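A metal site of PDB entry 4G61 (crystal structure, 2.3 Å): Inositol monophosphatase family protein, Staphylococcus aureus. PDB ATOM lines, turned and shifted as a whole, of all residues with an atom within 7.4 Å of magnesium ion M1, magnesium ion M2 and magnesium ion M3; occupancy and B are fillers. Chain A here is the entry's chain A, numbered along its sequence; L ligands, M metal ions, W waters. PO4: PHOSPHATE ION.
Within 4 Å of magnesium ion M1: Glu 76, Asp 94, Ile 96 and Asp 97.
Water W3 lies within hydrogen-bond range of OE2 of Glu 77 (2.6 Å), OD2 of Asp 53 (2.9 Å) and N of Ile 96 (3.3 Å).
Water W2 lies within hydrogen-bond range of OE2 of Glu 77 (2.5 Å), O of Leu 48 (3.0 Å) and NZ of Lys 42 (3.2 Å).
Water W4 bridges the side-chain carboxylate (OD1) of Asp 47 (2.7 Å) and the side-chain amino group (NZ) of Lys 42 (2.9 Å).
Water W5 bridges NE1 of Trp 214 (3.0 Å) and OD2 of Asp 215 (3.2 Å).
Residues that only touch magnesium ion M3: Lys 42 (3.8 Å) and Leu 48 (3.8 Å).
Three residues have an atom within 4 Å of magnesium ion M3: Lys 42, Leu 48 and Glu 76.
The nearest printed residue that does not touch magnesium ion M3 is Glu 77 (4.1 Å).
Magnesium ion M3 is bound by O1 of the ligand (1.9 Å).
Magnesium ion M3 is bound by water W6.
Water W2 is bound to magnesium ion M3 (2.1 Å).
Water W4 is bound to magnesium ion M3.
OE1 of Glu 76 binds magnesium ion M3 (2.2 Å).
Water W1 binds magnesium ion M3 (2.4 Å).
Magnesium ion M3 has six donor atoms within binding distance.
Within 4 Å of magnesium ion M2: Asp 94, Asp 97 and Asp 215.
Magnesium ion M2 is bound by O2 of the ligand (1.9 Å), OD1 of Asp 97 (2.0 Å), OD1 of Asp 215 (2.1 Å), O4 of the ligand (2.1 Å) and OD2 of Asp 94 (2.3 Å).
Magnesium ion M1 is bound by O4 of the ligand, OD1 of Asp 94, O of Ile 96, OE2 of Glu 76, water W3 and water W1.
The backbone NH (N) of Asp 94 lies within hydrogen-bond range of the backbone carbonyl oxygen (O) of Ile 112 (2.9 Å).
The side-chain carboxylate (OD2) of Asp 97 is in hydrogen-bond range of the backbone NH (N) of Cys 191 (3.1 Å).
N of Asp 97 sits at hydrogen-bond distance from O of Cys 110.
N of Glu 76 is in hydrogen-bond range of O of Met 93 (3.3 Å).
N of Glu 76 sits close to NE2 of Gln 57 (3.4 Å).
O of Asp 215 sits at hydrogen-bond distance from SG of Cys 191, at 3.4 Å.
The side-chain carboxylate (OD2) of Asp 215 is in hydrogen-bond range of the backbone NH (N) of Lys 212, at 2.8 Å.
The backbone NH (N) of Lys 42 lies within hydrogen-bond range of the backbone carbonyl oxygen (O) of Asp 47.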
ATOM      1  N   LYS A  42      -5.460 -15.480 -27.182  1.00  0.00           N
ATOM      2  CA  LYS A  42      -4.796 -14.173 -27.103  1.00  0.00           C
ATOM      3  C   LYS A  42      -3.524 -14.273 -26.253  1.00  0.00           C
ATOM      4  O   LYS A  42      -2.472 -14.751 -26.733  1.00  0.00           O
ATOM      5  CB  LYS A  42      -5.772 -13.077 -26.632  1.00  0.00           C
ATOM      6  CG  LYS A  42      -6.804 -12.743 -27.733  1.00  0.00           C
ATOM      7  CD  LYS A  42      -7.454 -11.341 -27.594  1.00  0.00           C
ATOM      8  CE  LYS A  42      -8.461 -11.302 -26.465  1.00  0.00           C
ATOM      9  NZ  LYS A  42      -8.863  -9.964 -26.035  1.00  0.00           N
ATOM     10  N   ASP A  47      -7.403 -17.449 -22.863  1.00  0.00           N
ATOM     11  CA  ASP A  47      -7.815 -16.072 -23.125  1.00  0.00           C
ATOM     12  C   ASP A  47      -8.409 -16.038 -24.536  1.00  0.00           C
ATOM     13  O   ASP A  47      -7.692 -15.805 -25.501  1.00  0.00           O
ATOM     14  CB  ASP A  47      -6.605 -15.136 -23.057  1.00  0.00           C
ATOM     15  CG  ASP A  47      -6.985 -13.674 -23.099  1.00  0.00           C
ATOM     16  OD1 ASP A  47      -8.188 -13.334 -22.834  1.00  0.00           O
ATOM     17  OD2 ASP A  47      -6.063 -12.860 -23.398  1.00  0.00           O
ATOM     18  N   LEU A  48      -9.714 -16.256 -24.636  1.00  0.00           N
ATOM     19  CA  LEU A  48     -10.369 -16.613 -25.893  1.00  0.00           C
ATOM     20  C   LEU A  48     -10.920 -15.432 -26.650  1.00  0.00           C
ATOM     21  O   LEU A  48     -11.444 -14.470 -26.068  1.00  0.00           O
ATOM     22  CB  LEU A  48     -11.539 -17.530 -25.589  1.00  0.00           C
ATOM     23  CG  LEU A  48     -11.362 -19.050 -25.501  1.00  0.00           C
ATOM     24  CD1 LEU A  48      -9.959 -19.537 -25.249  1.00  0.00           C
ATOM     25  CD2 LEU A  48     -12.382 -19.660 -24.554  1.00  0.00           C
ATOM     26  N   VAL A  49     -10.869 -15.548 -27.971  1.00  0.00           N
ATOM     27  CA  VAL A  49     -11.629 -14.684 -28.823  1.00  0.00           C
ATOM     28  C   VAL A  49     -12.308 -15.527 -29.926  1.00  0.00           C
ATOM     29  O   VAL A  49     -11.694 -16.467 -30.460  1.00  0.00           O
ATOM     30  CB  VAL A  49     -10.754 -13.496 -29.386  1.00  0.00           C
ATOM     31  CG1 VAL A  49      -9.623 -13.980 -30.332  1.00  0.00           C
ATOM     32  CG2 VAL A  49     -11.629 -12.479 -30.075  1.00  0.00           C
ATOM     33  N   ASP A  53     -17.094 -12.368 -31.353  1.00  0.00           N
ATOM     34  CA  ASP A  53     -16.435 -11.119 -30.933  1.00  0.00           C
ATOM     35  C   ASP A  53     -16.026 -10.309 -32.160  1.00  0.00           C
ATOM     36  O   ASP A  53     -16.429  -9.184 -32.278  1.00  0.00           O
ATOM     37  CB  ASP A  53     -15.176 -11.325 -30.049  1.00  0.00           C
ATOM     38  CG  ASP A  53     -15.353 -12.347 -28.931  1.00  0.00           C
ATOM     39  OD1 ASP A  53     -15.374 -13.570 -29.245  1.00  0.00           O
ATOM     40  OD2 ASP A  53     -15.446 -11.952 -27.734  1.00  0.00           O
ATOM     41  N   GLN A  57     -17.703  -6.523 -33.591  1.00  0.00           N
ATOM     42  CA  GLN A  57     -16.921  -5.301 -33.424  1.00  0.00           C
ATOM     43  C   GLN A  57     -16.632  -4.690 -34.794  1.00  0.00           C
ATOM     44  O   GLN A  57     -16.592  -3.469 -34.935  1.00  0.00           O
ATOM     45  CB  GLN A  57     -15.596  -5.586 -32.689  1.00  0.00           C
ATOM     46  CG  GLN A  57     -14.718  -4.375 -32.550  1.00  0.00           C
ATOM     47  CD  GLN A  57     -13.429  -4.649 -31.829  1.00  0.00           C
ATOM     48  OE1 GLN A  57     -12.349  -4.598 -32.407  1.00  0.00           O
ATOM     49  NE2 GLN A  57     -13.533  -4.921 -30.544  1.00  0.00           N
ATOM     50  N   GLU A  76     -11.974  -3.953 -27.630  1.00  0.00           N
ATOM     51  CA  GLU A  76     -11.166  -5.035 -27.165  1.00  0.00           C
ATOM     52  C   GLU A  76     -10.381  -5.753 -28.247  1.00  0.00           C
ATOM     53  O   GLU A  76      -9.217  -6.097 -28.042  1.00  0.00           O
ATOM     54  CB  GLU A  76     -12.025  -6.063 -26.428  1.00  0.00           C
ATOM     55  CG  GLU A  76     -11.141  -7.139 -25.781  1.00  0.00           C
ATOM     56  CD  GLU A  76     -11.931  -8.178 -25.028  1.00  0.00           C
ATOM     57  OE1 GLU A  76     -11.315  -9.201 -24.627  1.00  0.00           O
ATOM     58  OE2 GLU A  76     -13.173  -8.005 -24.915  1.00  0.00           O
ATOM     59  N   GLU A  77     -11.010  -5.998 -29.393  1.00  0.00           N
ATOM     60  CA  GLU A  77     -10.416  -6.945 -30.345  1.00  0.00           C
ATOM     61  C   GLU A  77      -9.693  -6.221 -31.471  1.00  0.00           C
ATOM     62  O   GLU A  77      -9.686  -6.662 -32.628  1.00  0.00           O
ATOM     63  CB  GLU A  77     -11.416  -7.999 -30.850  1.00  0.00           C
ATOM     64  CG  GLU A  77     -12.344  -8.607 -29.791  1.00  0.00           C
ATOM     65  CD  GLU A  77     -11.626  -9.432 -28.770  1.00  0.00           C
ATOM     66  OE1 GLU A  77     -10.408  -9.703 -28.961  1.00  0.00           O
ATOM     67  OE2 GLU A  77     -12.270  -9.758 -27.725  1.00  0.00           O
ATOM     68  N   MET A  93     -16.144  -0.148 -26.684  1.00  0.00           N
ATOM     69  CA  MET A  93     -16.887  -1.392 -26.911  1.00  0.00           C
ATOM     70  C   MET A  93     -16.202  -2.672 -26.438  1.00  0.00           C
ATOM     71  O   MET A  93     -15.029  -2.924 -26.754  1.00  0.00           O
ATOM     72  CB  MET A  93     -17.200  -1.555 -28.400  1.00  0.00           C
ATOM     73  CG  MET A  93     -18.025  -2.821 -28.694  1.00  0.00           C
ATOM     74  SD  MET A  93     -18.289  -2.976 -30.476  1.00  0.00           S
ATOM     75  CE  MET A  93     -20.008  -3.437 -30.460  1.00  0.00           C
ATOM     76  N   ASP A  94     -16.972  -3.510 -25.744  1.00  0.00           N
ATOM     77  CA  ASP A  94     -16.597  -4.894 -25.508  1.00  0.00           C
ATOM     78  C   ASP A  94     -17.578  -5.715 -26.363  1.00  0.00           C
ATOM     79  O   ASP A  94     -18.747  -5.831 -26.038  1.00  0.00           O
ATOM     80  CB  ASP A  94     -16.738  -5.216 -24.024  1.00  0.00           C
ATOM     81  CG  ASP A  94     -16.135  -6.574 -23.663  1.00  0.00           C
ATOM     82  OD1 ASP A  94     -15.982  -7.413 -24.572  1.00  0.00           O
ATOM     83  OD2 ASP A  94     -15.841  -6.814 -22.455  1.00  0.00           O
ATOM     84  N   PRO A  95     -17.094  -6.243 -27.494  1.00  0.00           N
ATOM     85  CA  PRO A  95     -18.032  -6.809 -28.452  1.00  0.00           C
ATOM     86  C   PRO A  95     -18.737  -8.049 -27.909  1.00  0.00           C
ATOM     87  O   PRO A  95     -19.945  -8.212 -28.130  1.00  0.00           O
ATOM     88  CB  PRO A  95     -17.148  -7.172 -29.643  1.00  0.00           C
ATOM     89  CG  PRO A  95     -15.740  -7.114 -29.130  1.00  0.00           C
ATOM     90  CD  PRO A  95     -15.695  -6.259 -27.969  1.00  0.00           C
ATOM     91  N   ILE A  96     -17.994  -8.898 -27.203  1.00  0.00           N
ATOM     92  CA  ILE A  96     -18.569  -9.919 -26.384  1.00  0.00           C
ATOM     93  C   ILE A  96     -17.867  -9.827 -25.032  1.00  0.00           C
ATOM     94  O   ILE A  96     -16.661 -10.032 -24.935  1.00  0.00           O
ATOM     95  CB  ILE A  96     -18.436 -11.342 -26.968  1.00  0.00           C
ATOM     96  CG1 ILE A  96     -19.313 -11.525 -28.231  1.00  0.00           C
ATOM     97  CG2 ILE A  96     -18.755 -12.391 -25.908  1.00  0.00           C
ATOM     98  CD1 ILE A  96     -20.781 -11.384 -27.994  1.00  0.00           C
ATOM     99  N   ASP A  97     -18.612  -9.445 -24.011  1.00  0.00           N
ATOM    100  CA  ASP A  97     -18.111  -9.507 -22.671  1.00  0.00           C
ATOM    101  C   ASP A  97     -18.578 -10.861 -22.058  1.00  0.00           C
ATOM    102  O   ASP A  97     -19.779 -11.119 -22.000  1.00  0.00           O
ATOM    103  CB  ASP A  97     -18.616  -8.338 -21.825  1.00  0.00           C
ATOM    104  CG  ASP A  97     -17.997  -8.342 -20.456  1.00  0.00           C
ATOM    105  OD1 ASP A  97     -16.753  -8.451 -20.437  1.00  0.00           O
ATOM    106  OD2 ASP A  97     -18.709  -8.276 -19.402  1.00  0.00           O
ATOM    107  N   GLY A  98     -17.623 -11.704 -21.633  1.00  0.00           N
ATOM    108  CA  GLY A  98     -17.973 -13.086 -21.256  1.00  0.00           C
ATOM    109  C   GLY A  98     -17.768 -14.099 -22.355  1.00  0.00           C
ATOM    110  O   GLY A  98     -18.570 -15.043 -22.530  1.00  0.00           O
ATOM    111  N   THR A  99     -16.677 -13.956 -23.088  1.00  0.00           N
ATOM    112  CA  THR A  99     -16.425 -14.884 -24.209  1.00  0.00           C
ATOM    113  C   THR A  99     -16.342 -16.338 -23.682  1.00  0.00           C
ATOM    114  O   THR A  99     -16.835 -17.278 -24.304  1.00  0.00           O
ATOM    115  CB  THR A  99     -15.120 -14.480 -24.964  1.00  0.00           C
ATOM    116  OG1 THR A  99     -15.210 -13.084 -25.291  1.00  0.00           O
ATOM    117  CG2 THR A  99     -14.972 -15.249 -26.206  1.00  0.00           C
ATOM    118  N   ALA A 100     -15.726 -16.531 -22.516  1.00  0.00           N
ATOM    119  CA  ALA A 100     -15.614 -17.872 -22.027  1.00  0.00           C
ATOM    120  C   ALA A 100     -17.062 -18.453 -21.886  1.00  0.00           C
ATOM    121  O   ALA A 100     -17.334 -19.578 -22.276  1.00  0.00           O
ATOM    122  CB  ALA A 100     -14.843 -17.855 -20.715  1.00  0.00           C
ATOM    123  N   CYS A 110     -22.654 -10.716 -22.909  1.00  0.00           N
ATOM    124  CA  CYS A 110     -23.409  -9.541 -23.316  1.00  0.00           C
ATOM    125  C   CYS A 110     -22.496  -8.706 -24.180  1.00  0.00           C
ATOM    126  O   CYS A 110     -21.297  -9.020 -24.326  1.00  0.00           O
ATOM    127  CB  CYS A 110     -23.784  -8.719 -22.109  1.00  0.00           C
ATOM    128  SG  CYS A 110     -22.292  -8.179 -21.103  1.00  0.00           S
ATOM    129  N   ILE A 112     -21.200  -4.793 -24.576  1.00  0.00           N
ATOM    130  CA  ILE A 112     -21.028  -3.557 -23.834  1.00  0.00           C
ATOM    131  C   ILE A 112     -20.637  -2.390 -24.753  1.00  0.00           C
ATOM    132  O   ILE A 112     -19.690  -2.474 -25.531  1.00  0.00           O
ATOM    133  CB  ILE A 112     -20.037  -3.755 -22.659  1.00  0.00           C
ATOM    134  CG1 ILE A 112     -20.527  -4.880 -21.712  1.00  0.00           C
ATOM    135  CG2 ILE A 112     -19.797  -2.406 -21.885  1.00  0.00           C
ATOM    136  CD1 ILE A 112     -19.522  -5.277 -20.560  1.00  0.00           C
ATOM    137  N   ALA A 190     -19.644 -12.644 -16.561  1.00  0.00           N
ATOM    138  CA  ALA A 190     -19.435 -11.503 -17.404  1.00  0.00           C
ATOM    139  C   ALA A 190     -19.537 -10.227 -16.587  1.00  0.00           C
ATOM    140  O   ALA A 190     -20.590  -9.924 -16.048  1.00  0.00           O
ATOM    141  CB  ALA A 190     -20.508 -11.451 -18.575  1.00  0.00           C
ATOM    142  N   CYS A 191     -18.482  -9.433 -16.554  1.00  0.00           N
ATOM    143  CA  CYS A 191     -18.467  -8.169 -15.788  1.00  0.00           C
ATOM    144  C   CYS A 191     -19.716  -7.280 -15.994  1.00  0.00           C
ATOM    145  O   CYS A 191     -20.237  -6.697 -15.038  1.00  0.00           O
ATOM    146  CB  CYS A 191     -17.261  -7.368 -16.222  1.00  0.00           C
ATOM    147  SG  CYS A 191     -16.969  -5.929 -15.220  1.00  0.00           S
ATOM    148  N   GLY A 192     -20.127  -7.117 -17.252  1.00  0.00           N
ATOM    149  CA  GLY A 192     -21.301  -6.296 -17.561  1.00  0.00           C
ATOM    150  C   GLY A 192     -22.544  -6.865 -16.927  1.00  0.00           C
ATOM    151  O   GLY A 192     -23.358  -6.139 -16.427  1.00  0.00           O
ATOM    152  N   ASN A 208     -13.946  -6.604  -9.929  1.00  0.00           N
ATOM    153  CA  ASN A 208     -13.017  -7.158 -10.958  1.00  0.00           C
ATOM    154  C   ASN A 208     -11.705  -6.497 -10.687  1.00  0.00           C
ATOM    155  O   ASN A 208     -11.616  -5.285 -10.788  1.00  0.00           O
ATOM    156  CB  ASN A 208     -13.441  -6.821 -12.387  1.00  0.00           C
ATOM    157  CG  ASN A 208     -12.543  -7.524 -13.488  1.00  0.00           C
ATOM    158  OD1 ASN A 208     -11.328  -7.721 -13.322  1.00  0.00           O
ATOM    159  ND2 ASN A 208     -13.176  -7.865 -14.617  1.00  0.00           N
ATOM    160  N   LYS A 212     -10.229  -4.366 -18.195  1.00  0.00           N
ATOM    161  CA  LYS A 212      -9.878  -3.447 -19.269  1.00  0.00           C
ATOM    162  C   LYS A 212     -10.948  -2.328 -19.374  1.00  0.00           C
ATOM    163  O   LYS A 212     -12.039  -2.486 -18.825  1.00  0.00           O
ATOM    164  CB  LYS A 212      -9.716  -4.256 -20.550  1.00  0.00           C
ATOM    165  CG  LYS A 212      -8.570  -5.351 -20.393  1.00  0.00           C
ATOM    166  CD  LYS A 212      -7.178  -4.733 -20.620  1.00  0.00           C
ATOM    167  CE  LYS A 212      -6.070  -5.323 -19.692  1.00  0.00           C
ATOM    168  NZ  LYS A 212      -6.251  -6.781 -19.380  1.00  0.00           N
ATOM    169  N   TRP A 214     -13.016  -1.471 -21.645  1.00  0.00           N
ATOM    170  CA  TRP A 214     -14.268  -2.009 -22.232  1.00  0.00           C
ATOM    171  C   TRP A 214     -15.104  -2.914 -21.308  1.00  0.00           C
ATOM    172  O   TRP A 214     -16.300  -3.070 -21.524  1.00  0.00           O
ATOM    173  CB  TRP A 214     -13.967  -2.704 -23.604  1.00  0.00           C
ATOM    174  CG  TRP A 214     -12.779  -3.681 -23.544  1.00  0.00           C
ATOM    175  CD1 TRP A 214     -12.817  -4.959 -23.080  1.00  0.00           C
ATOM    176  CD2 TRP A 214     -11.387  -3.428 -23.925  1.00  0.00           C
ATOM    177  NE1 TRP A 214     -11.550  -5.527 -23.177  1.00  0.00           N
ATOM    178  CE2 TRP A 214     -10.660  -4.622 -23.691  1.00  0.00           C
ATOM    179  CE3 TRP A 214     -10.711  -2.329 -24.453  1.00  0.00           C
ATOM    180  CZ2 TRP A 214      -9.279  -4.748 -23.952  1.00  0.00           C
ATOM    181  CZ3 TRP A 214      -9.328  -2.436 -24.701  1.00  0.00           C
ATOM    182  CH2 TRP A 214      -8.624  -3.638 -24.444  1.00  0.00           C
ATOM    183  N   ASP A 215     -14.483  -3.515 -20.286  1.00  0.00           N
ATOM    184  CA  ASP A 215     -15.238  -4.270 -19.248  1.00  0.00           C
ATOM    185  C   ASP A 215     -16.128  -3.401 -18.374  1.00  0.00           C
ATOM    186  O   ASP A 215     -17.156  -3.859 -17.887  1.00  0.00           O
ATOM    187  CB  ASP A 215     -14.289  -5.072 -18.371  1.00  0.00           C
ATOM    188  CG  ASP A 215     -13.466  -6.038 -19.178  1.00  0.00           C
ATOM    189  OD1 ASP A 215     -14.030  -6.704 -20.055  1.00  0.00           O
ATOM    190  OD2 ASP A 215     -12.254  -6.128 -18.944  1.00  0.00           O
ATOM    191  N   ILE A 216     -15.763  -2.144 -18.201  1.00  0.00           N
ATOM    192  CA  ILE A 216     -16.483  -1.287 -17.259  1.00  0.00           C
ATOM    193  C   ILE A 216     -16.970   0.043 -17.856  1.00  0.00           C
ATOM    194  O   ILE A 216     -17.553   0.854 -17.131  1.00  0.00           O
ATOM    195  CB  ILE A 216     -15.628  -0.980 -16.011  1.00  0.00           C
ATOM    196  CG1 ILE A 216     -14.329  -0.230 -16.410  1.00  0.00           C
ATOM    197  CG2 ILE A 216     -15.369  -2.250 -15.267  1.00  0.00           C
ATOM    198  CD1 ILE A 216     -13.536   0.364 -15.229  1.00  0.00           C
HETATM  199  P   PO4 L   1     -14.020 -10.521 -22.053  1.00  0.00           P
HETATM  200  O1  PO4 L   1     -12.531 -10.627 -22.431  1.00  0.00           O
HETATM  201  O2  PO4 L   1     -14.078  -9.975 -20.589  1.00  0.00           O
HETATM  202  O3  PO4 L   1     -14.631 -11.885 -22.199  1.00  0.00           O
HETATM  203  O4  PO4 L   1     -14.786  -9.516 -22.859  1.00  0.00           O
HETATM  204 MG    MG M   1     -14.913  -9.049 -24.714  1.00  0.00          MG
HETATM  205 MG    MG M   2     -14.862  -8.331 -21.087  1.00  0.00          MG
HETATM  206 MG    MG M   3     -11.697 -11.274 -23.955  1.00  0.00          MG
HETATM  207  O   HOH W   1     -13.956 -11.128 -24.702  1.00  0.00           O
HETATM  208  O   HOH W   2     -11.648 -11.516 -26.067  1.00  0.00           O
HETATM  209  O   HOH W   3     -14.681  -9.249 -26.946  1.00  0.00           O
HETATM  210  O   HOH W   4      -9.594 -11.148 -23.506  1.00  0.00           O
HETATM  211  O   HOH W   5     -11.857  -7.986 -21.487  1.00  0.00           O
HETATM  212  O   HOH W   6     -11.997 -13.337 -23.573  1.00  0.00           O
